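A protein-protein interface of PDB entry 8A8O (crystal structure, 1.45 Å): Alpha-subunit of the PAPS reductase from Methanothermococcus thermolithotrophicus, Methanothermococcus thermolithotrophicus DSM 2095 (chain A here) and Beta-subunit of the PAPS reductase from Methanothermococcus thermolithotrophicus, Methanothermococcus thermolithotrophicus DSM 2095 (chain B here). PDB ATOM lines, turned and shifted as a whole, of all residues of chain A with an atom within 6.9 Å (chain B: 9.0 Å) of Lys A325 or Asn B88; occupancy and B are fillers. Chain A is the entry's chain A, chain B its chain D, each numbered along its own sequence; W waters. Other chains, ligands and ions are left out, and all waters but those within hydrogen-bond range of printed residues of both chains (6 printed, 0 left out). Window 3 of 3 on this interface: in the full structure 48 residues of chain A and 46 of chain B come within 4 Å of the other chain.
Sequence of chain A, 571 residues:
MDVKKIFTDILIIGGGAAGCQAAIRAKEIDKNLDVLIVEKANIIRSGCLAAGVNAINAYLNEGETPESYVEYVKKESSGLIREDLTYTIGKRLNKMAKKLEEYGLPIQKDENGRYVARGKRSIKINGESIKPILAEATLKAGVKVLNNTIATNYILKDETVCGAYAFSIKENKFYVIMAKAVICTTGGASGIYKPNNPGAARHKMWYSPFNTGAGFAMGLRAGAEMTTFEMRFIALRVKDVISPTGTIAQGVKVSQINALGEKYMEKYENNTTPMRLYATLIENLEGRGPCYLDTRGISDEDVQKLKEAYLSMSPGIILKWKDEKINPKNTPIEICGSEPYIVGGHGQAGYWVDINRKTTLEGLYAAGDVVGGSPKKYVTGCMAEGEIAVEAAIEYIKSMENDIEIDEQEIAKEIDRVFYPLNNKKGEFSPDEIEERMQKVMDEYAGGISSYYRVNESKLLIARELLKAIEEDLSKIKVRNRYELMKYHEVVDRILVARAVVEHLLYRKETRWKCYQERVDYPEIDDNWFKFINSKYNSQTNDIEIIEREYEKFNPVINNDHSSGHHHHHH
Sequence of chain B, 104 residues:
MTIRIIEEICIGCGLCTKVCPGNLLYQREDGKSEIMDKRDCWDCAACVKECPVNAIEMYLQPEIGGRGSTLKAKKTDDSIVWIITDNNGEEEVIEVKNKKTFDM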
ATOM      1  N   LEU A 319     -26.798   9.385  20.654  1.00  0.00           N
ATOM      2  CA  LEU A 319     -26.243   8.033  20.700  1.00  0.00           C
ATOM      3  C   LEU A 319     -25.140   7.934  21.740  1.00  0.00           C
ATOM      4  O   LEU A 319     -25.047   6.930  22.450  1.00  0.00           O
ATOM      5  CB  LEU A 319     -25.719   7.660  19.323  1.00  0.00           C
ATOM      6  CG  LEU A 319     -26.799   7.506  18.251  1.00  0.00           C
ATOM      7  CD1 LEU A 319     -26.158   7.255  16.906  1.00  0.00           C
ATOM      8  CD2 LEU A 319     -27.734   6.366  18.628  1.00  0.00           C
ATOM      9  N   LYS A 320     -24.293   8.959  21.843  1.00  0.00           N
ATOM     10  CA  LYS A 320     -23.268   8.954  22.875  1.00  0.00           C
ATOM     11  C   LYS A 320     -23.892   8.895  24.255  1.00  0.00           C
ATOM     12  O   LYS A 320     -23.443   8.130  25.119  1.00  0.00           O
ATOM     13  CB  LYS A 320     -22.390  10.193  22.751  1.00  0.00           C
ATOM     14  CG  LYS A 320     -21.273  10.229  23.780  1.00  0.00           C
ATOM     15  CD  LYS A 320     -20.463  11.514  23.666  1.00  0.00           C
ATOM     16  CE  LYS A 320     -19.541  11.705  24.867  1.00  0.00           C
ATOM     17  NZ  LYS A 320     -18.269  10.941  24.720  1.00  0.00           N
ATOM     18  N   TRP A 321     -24.939   9.691  24.481  1.00  0.00           N
ATOM     19  CA  TRP A 321     -25.571   9.703  25.793  1.00  0.00           C
ATOM     20  C   TRP A 321     -26.190   8.351  26.115  1.00  0.00           C
ATOM     21  O   TRP A 321     -26.138   7.898  27.265  1.00  0.00           O
ATOM     22  CB  TRP A 321     -26.610  10.815  25.880  1.00  0.00           C
ATOM     23  CG  TRP A 321     -26.013  12.180  25.939  1.00  0.00           C
ATOM     24  CD1 TRP A 321     -24.698  12.494  26.061  1.00  0.00           C
ATOM     25  CD2 TRP A 321     -26.718  13.420  25.861  1.00  0.00           C
ATOM     26  NE1 TRP A 321     -24.531  13.861  26.057  1.00  0.00           N
ATOM     27  CE2 TRP A 321     -25.761  14.452  25.953  1.00  0.00           C
ATOM     28  CE3 TRP A 321     -28.069  13.761  25.736  1.00  0.00           C
ATOM     29  CZ2 TRP A 321     -26.109  15.797  25.912  1.00  0.00           C
ATOM     30  CZ3 TRP A 321     -28.409  15.102  25.683  1.00  0.00           C
ATOM     31  CH2 TRP A 321     -27.433  16.103  25.772  1.00  0.00           C
ATOM     32  N   LYS A 322     -26.792   7.690  25.117  1.00  0.00           N
ATOM     33  CA  LYS A 322     -27.398   6.383  25.367  1.00  0.00           C
ATOM     34  C   LYS A 322     -26.340   5.313  25.610  1.00  0.00           C
ATOM     35  O   LYS A 322     -26.505   4.464  26.497  1.00  0.00           O
ATOM     36  CB  LYS A 322     -28.262   5.972  24.178  1.00  0.00           C
ATOM     37  CG  LYS A 322     -29.560   6.733  24.038  1.00  0.00           C
ATOM     38  CD  LYS A 322     -30.666   6.147  24.868  1.00  0.00           C
ATOM     39  CE  LYS A 322     -31.866   7.080  24.848  1.00  0.00           C
ATOM     40  NZ  LYS A 322     -33.077   6.423  25.393  1.00  0.00           N
ATOM     41  N   ASP A 323     -25.266   5.321  24.815  1.00  0.00           N
ATOM     42  CA  ASP A 323     -24.202   4.336  24.976  1.00  0.00           C
ATOM     43  C   ASP A 323     -23.510   4.480  26.327  1.00  0.00           C
ATOM     44  O   ASP A 323     -23.249   3.479  27.010  1.00  0.00           O
ATOM     45  CB  ASP A 323     -23.158   4.527  23.868  1.00  0.00           C
ATOM     46  CG  ASP A 323     -23.520   3.815  22.569  1.00  0.00           C
ATOM     47  OD1 ASP A 323     -24.414   2.948  22.575  1.00  0.00           O
ATOM     48  OD2 ASP A 323     -22.874   4.100  21.537  1.00  0.00           O
ATOM     49  N   GLU A 324     -23.214   5.718  26.733  1.00  0.00           N
ATOM     50  CA  GLU A 324     -22.422   6.003  27.922  1.00  0.00           C
ATOM     51  C   GLU A 324     -23.268   6.327  29.140  1.00  0.00           C
ATOM     52  O   GLU A 324     -22.711   6.649  30.196  1.00  0.00           O
ATOM     53  CB  GLU A 324     -21.429   7.142  27.621  1.00  0.00           C
ATOM     54  CG  GLU A 324     -20.620   6.900  26.347  1.00  0.00           C
ATOM     55  CD  GLU A 324     -19.393   7.796  26.210  1.00  0.00           C
ATOM     56  OE1 GLU A 324     -19.354   8.872  26.839  1.00  0.00           O
ATOM     57  OE2 GLU A 324     -18.460   7.418  25.458  1.00  0.00           O
ATOM     58  N   LYS A 325     -24.591   6.213  29.035  1.00  0.00           N
ATOM     59  CA  LYS A 325     -25.487   6.371  30.179  1.00  0.00           C
ATOM     60  C   LYS A 325     -25.364   7.767  30.785  1.00  0.00           C
ATOM     61  O   LYS A 325     -25.276   7.940  32.003  1.00  0.00           O
ATOM     62  CB  LYS A 325     -25.245   5.284  31.230  1.00  0.00           C
ATOM     63  CG  LYS A 325     -25.108   3.857  30.682  1.00  0.00           C
ATOM     64  CD  LYS A 325     -26.237   3.473  29.733  1.00  0.00           C
ATOM     65  CE  LYS A 325     -25.916   2.176  28.991  1.00  0.00           C
ATOM     66  NZ  LYS A 325     -27.111   1.612  28.302  1.00  0.00           N
ATOM     67  N   ILE A 326     -25.362   8.774  29.920  1.00  0.00           N
ATOM     68  CA  ILE A 326     -25.275  10.165  30.344  1.00  0.00           C
ATOM     69  C   ILE A 326     -26.678  10.756  30.330  1.00  0.00           C
ATOM     70  O   ILE A 326     -27.314  10.852  29.273  1.00  0.00           O
ATOM     71  CB  ILE A 326     -24.341  10.960  29.421  1.00  0.00           C
ATOM     72  CG1 ILE A 326     -22.898  10.492  29.609  1.00  0.00           C
ATOM     73  CG2 ILE A 326     -24.452  12.456  29.709  1.00  0.00           C
ATOM     74  CD1 ILE A 326     -21.982  10.931  28.502  1.00  0.00           C
ATOM     75  N   ASN A 327     -27.164  11.160  31.501  1.00  0.00           N
ATOM     76  CA  ASN A 327     -28.336  12.019  31.586  1.00  0.00           C
ATOM     77  C   ASN A 327     -27.849  13.400  31.995  1.00  0.00           C
ATOM     78  O   ASN A 327     -27.308  13.549  33.104  1.00  0.00           O
ATOM     79  CB  ASN A 327     -29.355  11.503  32.596  1.00  0.00           C
ATOM     80  CG  ASN A 327     -30.629  12.331  32.599  1.00  0.00           C
ATOM     81  OD1 ASN A 327     -30.592  13.535  32.367  1.00  0.00           O
ATOM     82  ND2 ASN A 327     -31.757  11.695  32.881  1.00  0.00           N
ATOM     83  N   THR A 331     -25.160  14.334  34.974  1.00  0.00           N
ATOM     84  CA  THR A 331     -23.778  14.296  34.526  1.00  0.00           C
ATOM     85  C   THR A 331     -23.548  15.463  33.574  1.00  0.00           C
ATOM     86  O   THR A 331     -24.300  15.620  32.595  1.00  0.00           O
ATOM     87  CB  THR A 331     -23.540  12.970  33.784  1.00  0.00           C
ATOM     88  OG1 THR A 331     -23.868  11.869  34.640  1.00  0.00           O
ATOM     89  CG2 THR A 331     -22.094  12.842  33.334  1.00  0.00           C
ATOM     90  N   GLY B  65     -15.864   4.518  21.038  1.00  0.00           N
ATOM     91  CA  GLY B  65     -16.698   4.280  22.202  1.00  0.00           C
ATOM     92  C   GLY B  65     -18.132   3.904  21.910  1.00  0.00           C
ATOM     93  O   GLY B  65     -18.917   3.760  22.858  1.00  0.00           O
ATOM     94  N   ARG B  67     -21.275   1.664  21.489  1.00  0.00           N
ATOM     95  CA  ARG B  67     -21.615   0.407  22.152  1.00  0.00           C
ATOM     96  C   ARG B  67     -22.808  -0.291  21.510  1.00  0.00           C
ATOM     97  O   ARG B  67     -23.279  -1.315  22.034  1.00  0.00           O
ATOM     98  CB  ARG B  67     -21.868   0.625  23.645  1.00  0.00           C
ATOM     99  CG  ARG B  67     -20.715   1.282  24.389  1.00  0.00           C
ATOM    100  CD  ARG B  67     -20.904   1.218  25.904  1.00  0.00           C
ATOM    101  NE  ARG B  67     -21.003  -0.149  26.400  1.00  0.00           N
ATOM    102  CZ  ARG B  67     -21.564  -0.498  27.549  1.00  0.00           C
ATOM    103  NH1 ARG B  67     -22.055   0.407  28.383  1.00  0.00           N
ATOM    104  NH2 ARG B  67     -21.640  -1.788  27.870  1.00  0.00           N
ATOM    105  N   GLY B  68     -23.325   0.244  20.406  1.00  0.00           N
ATOM    106  CA  GLY B  68     -24.411  -0.389  19.690  1.00  0.00           C
ATOM    107  C   GLY B  68     -25.726   0.355  19.666  1.00  0.00           C
ATOM    108  O   GLY B  68     -26.657  -0.125  19.015  1.00  0.00           O
ATOM    109  N   SER B  69     -25.856   1.487  20.358  1.00  0.00           N
ATOM    110  CA  SER B  69     -27.082   2.271  20.237  1.00  0.00           C
ATOM    111  C   SER B  69     -27.252   2.732  18.790  1.00  0.00           C
ATOM    112  O   SER B  69     -26.276   3.025  18.095  1.00  0.00           O
ATOM    113  CB  SER B  69     -27.016   3.517  21.119  1.00  0.00           C
ATOM    114  OG  SER B  69     -27.130   3.190  22.489  1.00  0.00           O
ATOM    115  N   THR B  70     -28.500   2.811  18.338  1.00  0.00           N
ATOM    116  CA  THR B  70     -28.790   3.211  16.967  1.00  0.00           C
ATOM    117  C   THR B  70     -29.917   4.228  16.909  1.00  0.00           C
ATOM    118  O   THR B  70     -30.762   4.319  17.808  1.00  0.00           O
ATOM    119  CB  THR B  70     -29.186   2.004  16.089  1.00  0.00           C
ATOM    120  OG1 THR B  70     -30.471   1.514  16.511  1.00  0.00           O
ATOM    121  CG2 THR B  70     -28.160   0.906  16.183  1.00  0.00           C
ATOM    122  N   THR B  85     -32.702   3.366  19.765  1.00  0.00           N
ATOM    123  CA  THR B  85     -32.532   2.083  20.436  1.00  0.00           C
ATOM    124  C   THR B  85     -31.195   2.047  21.156  1.00  0.00           C
ATOM    125  O   THR B  85     -30.153   2.306  20.548  1.00  0.00           O
ATOM    126  CB  THR B  85     -32.608   0.933  19.429  1.00  0.00           C
ATOM    127  OG1 THR B  85     -33.724   1.138  18.554  1.00  0.00           O
ATOM    128  CG2 THR B  85     -32.767  -0.395  20.156  1.00  0.00           C
ATOM    129  N   ASP B  86     -31.210   1.722  22.445  1.00  0.00           N
ATOM    130  CA  ASP B  86     -29.964   1.754  23.198  1.00  0.00           C
ATOM    131  C   ASP B  86     -29.208   0.443  23.018  1.00  0.00           C
ATOM    132  O   ASP B  86     -29.610  -0.446  22.261  1.00  0.00           O
ATOM    133  CB  ASP B  86     -30.197   2.194  24.641  1.00  0.00           C
ATOM    134  CG  ASP B  86     -30.682   1.089  25.539  1.00  0.00           C
ATOM    135  OD1 ASP B  86     -30.891  -0.059  25.079  1.00  0.00           O
ATOM    136  OD2 ASP B  86     -30.855   1.387  26.742  1.00  0.00           O
ATOM    137  N   ASN B  87     -28.063   0.342  23.687  1.00  0.00           N
ATOM    138  CA  ASN B  87     -27.175  -0.777  23.429  1.00  0.00           C
ATOM    139  C   ASN B  87     -27.736  -2.091  23.950  1.00  0.00           C
ATOM    140  O   ASN B  87     -27.207  -3.147  23.592  1.00  0.00           O
ATOM    141  CB  ASN B  87     -25.780  -0.510  24.005  1.00  0.00           C
ATOM    142  CG  ASN B  87     -25.793  -0.309  25.502  1.00  0.00           C
ATOM    143  OD1 ASN B  87     -26.584   0.470  26.027  1.00  0.00           O
ATOM    144  ND2 ASN B  87     -24.921  -1.031  26.204  1.00  0.00           N
ATOM    145  N   ASN B  88     -28.784  -2.050  24.775  1.00  0.00           N
ATOM    146  CA  ASN B  88     -29.458  -3.243  25.263  1.00  0.00           C
ATOM    147  C   ASN B  88     -30.791  -3.497  24.572  1.00  0.00           C
ATOM    148  O   ASN B  88     -31.539  -4.387  24.993  1.00  0.00           O
ATOM    149  CB  ASN B  88     -29.647  -3.142  26.778  1.00  0.00           C
ATOM    150  CG  ASN B  88     -28.331  -3.001  27.520  1.00  0.00           C
ATOM    151  OD1 ASN B  88     -27.392  -3.774  27.297  1.00  0.00           O
ATOM    152  ND2 ASN B  88     -28.234  -1.983  28.370  1.00  0.00           N
ATOM    153  N   GLY B  89     -31.108  -2.742  23.525  1.00  0.00           N
ATOM    154  CA  GLY B  89     -32.328  -2.956  22.780  1.00  0.00           C
ATOM    155  C   GLY B  89     -33.520  -2.133  23.222  1.00  0.00           C
ATOM    156  O   GLY B  89     -34.580  -2.233  22.595  1.00  0.00           O
ATOM    157  N   GLU B  90     -33.384  -1.325  24.269  1.00  0.00           N
ATOM    158  CA  GLU B  90     -34.500  -0.514  24.739  1.00  0.00           C
ATOM    159  C   GLU B  90     -34.763   0.628  23.760  1.00  0.00           C
ATOM    160  O   GLU B  90     -33.838   1.299  23.306  1.00  0.00           O
ATOM    161  CB  GLU B  90     -34.183   0.061  26.119  1.00  0.00           C
ATOM    162  CG  GLU B  90     -34.240  -0.954  27.253  1.00  0.00           C
ATOM    163  CD  GLU B  90     -35.619  -1.565  27.407  1.00  0.00           C
ATOM    164  OE1 GLU B  90     -35.819  -2.705  26.939  1.00  0.00           O
ATOM    165  OE2 GLU B  90     -36.505  -0.896  27.984  1.00  0.00           O
ATOM    166  N   GLU B  91     -36.032   0.855  23.447  1.00  0.00           N
ATOM    167  CA  GLU B  91     -36.423   1.756  22.374  1.00  0.00           C
ATOM    168  C   GLU B  91     -37.124   2.977  22.950  1.00  0.00           C
ATOM    169  O   GLU B  91     -37.950   2.863  23.858  1.00  0.00           O
ATOM    170  CB  GLU B  91     -37.364   1.009  21.425  1.00  0.00           C
ATOM    171  CG  GLU B  91     -37.464   1.578  20.047  1.00  0.00           C
ATOM    172  CD  GLU B  91     -38.319   0.722  19.135  1.00  0.00           C
ATOM    173  OE1 GLU B  91     -37.801  -0.291  18.616  1.00  0.00           O
ATOM    174  OE2 GLU B  91     -39.508   1.059  18.948  1.00  0.00           O
HETATM  175  O   HOH W   1     -20.524   6.219  22.587  1.00  0.00           O
HETATM  176  O   HOH W   2     -33.526   4.142  23.908  1.00  0.00           O
HETATM  177  O   HOH W   3     -18.069   4.468  25.296  1.00  0.00           O
HETATM  178  O   HOH W   4     -21.129   2.859  28.927  1.00  0.00           O
HETATM  179  O   HOH W   5     -29.102   3.692  27.597  1.00  0.00           O
HETATM  180  O   HOH W   6     -23.838   3.804  18.869  1.00  0.00           O
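Lys A325 touches two residues of chain B.
Of the printed residues of chain A, Asn B88 touches Lys A325 (3.8 Å).
Of the printed residues of chain B, Asp A323 touches Arg B67 (2.9 Å), Gly B68 (3.6 Å), Ser B69 (2.7 Å) and Asn B87 (3.98 Å).
Printed residues of chain B within 4 Å of Lys A322: Ser B69 and Asp B86.
Of the printed residues of chain A, Asp B86 touches Lys A322 (3.99 Å).
Printed residues of chain B within 4 Å of Leu A319: Ser B69 and Thr B70.
Glu A324 touches none of the printed residues of chain B.
Thr B85 touches none of the printed residues of chain A.
The backbone carbonyl oxygen (O) of Lys A322 sits close to the side-chain amino group (NZ) of Lys A325.
OG of Ser B69 lies within hydrogen-bond range of N of Asn B87, 3.2 Å away.
The backbone carbonyl oxygen (O) of Thr B85 sits at hydrogen-bond distance from the backbone NH (N) of Thr B70, 2.8 Å away.
The side-chain carboxylate (OD1) of Asp B86 lies within hydrogen-bond range of the backbone NH (N) of Asn B88 (2.9 Å).
The side-chain carboxylate of Asp B86 lies within hydrogen-bond range of the backbone NH of Gly B89 (3.1 Å).
OD1 of Asp B86 sits at hydrogen-bond distance from N of Glu B90 (2.9 Å).
Water W6 lies within hydrogen-bond range of the backbone carbonyl oxygen (O) of Ser B69 (2.7 Å) and the side-chain carboxylate (OD2) of Asp A323 (2.9 Å).
Water W4 lies within hydrogen-bond range of the guanidinium group (NH1) of Arg B67 (2.7 Å) and the backbone carbonyl oxygen (O) of Asp A323 (2.9 Å).
Water W3 bridges O of Gly B65 (2.7 Å) and OE2 of Glu A324 (3.0 Å).
Water W2 lies within hydrogen-bond range of NZ of Lys A322 (2.8 Å) and O of Glu B90 (2.9 Å).
Water W5 lies within hydrogen-bond range of the backbone carbonyl oxygen of Lys A322 (2.9 Å), the side-chain amino group of Lys A325 (3.0 Å) and the side-chain carboxylate of Asp B86 (3.0 Å).
Water W1 bridges O of Gly B65 and OD2 of Asp A323.
Among the printed residues, merely in contact across the chains: Lys A322 with Ser B69, Leu A319 with Thr B70, Asp A323 with Gly B68, Leu A319 with Ser B69, Lys A325 with Asn B88, Asp A323 with Asn B87 and Lys A322 with Asp B86.
Printed residues of chain B that touch a printed residue of chain A: Arg B67, Gly B68, Ser B69, Thr B70, Asp B86, Asn B87 and Asn B88.
Hydrophobic or aromatic side chains of chain A within 4 Å of the printed part of chain B: Leu A319.
Among the printed residues, 10 pairs touch across the chains.
Among the printed residues, no Asp or Glu carboxylate lies within 4 Å of a Lys or Arg side-chain nitrogen of the other chain.
The side-chain carboxylate of Asp A323 sits at hydrogen-bond distance from the backbone NH of Arg B67 (2.9 Å).
OG of Ser B69 lies within hydrogen-bond range of OD1 of Asp A323, at 2.7 Å.
The side-chain amino group (NZ) of Lys A325 is in hydrogen-bond range of the side-chain amide oxygen (OD1) of Asn B87, at 2.6 Å.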
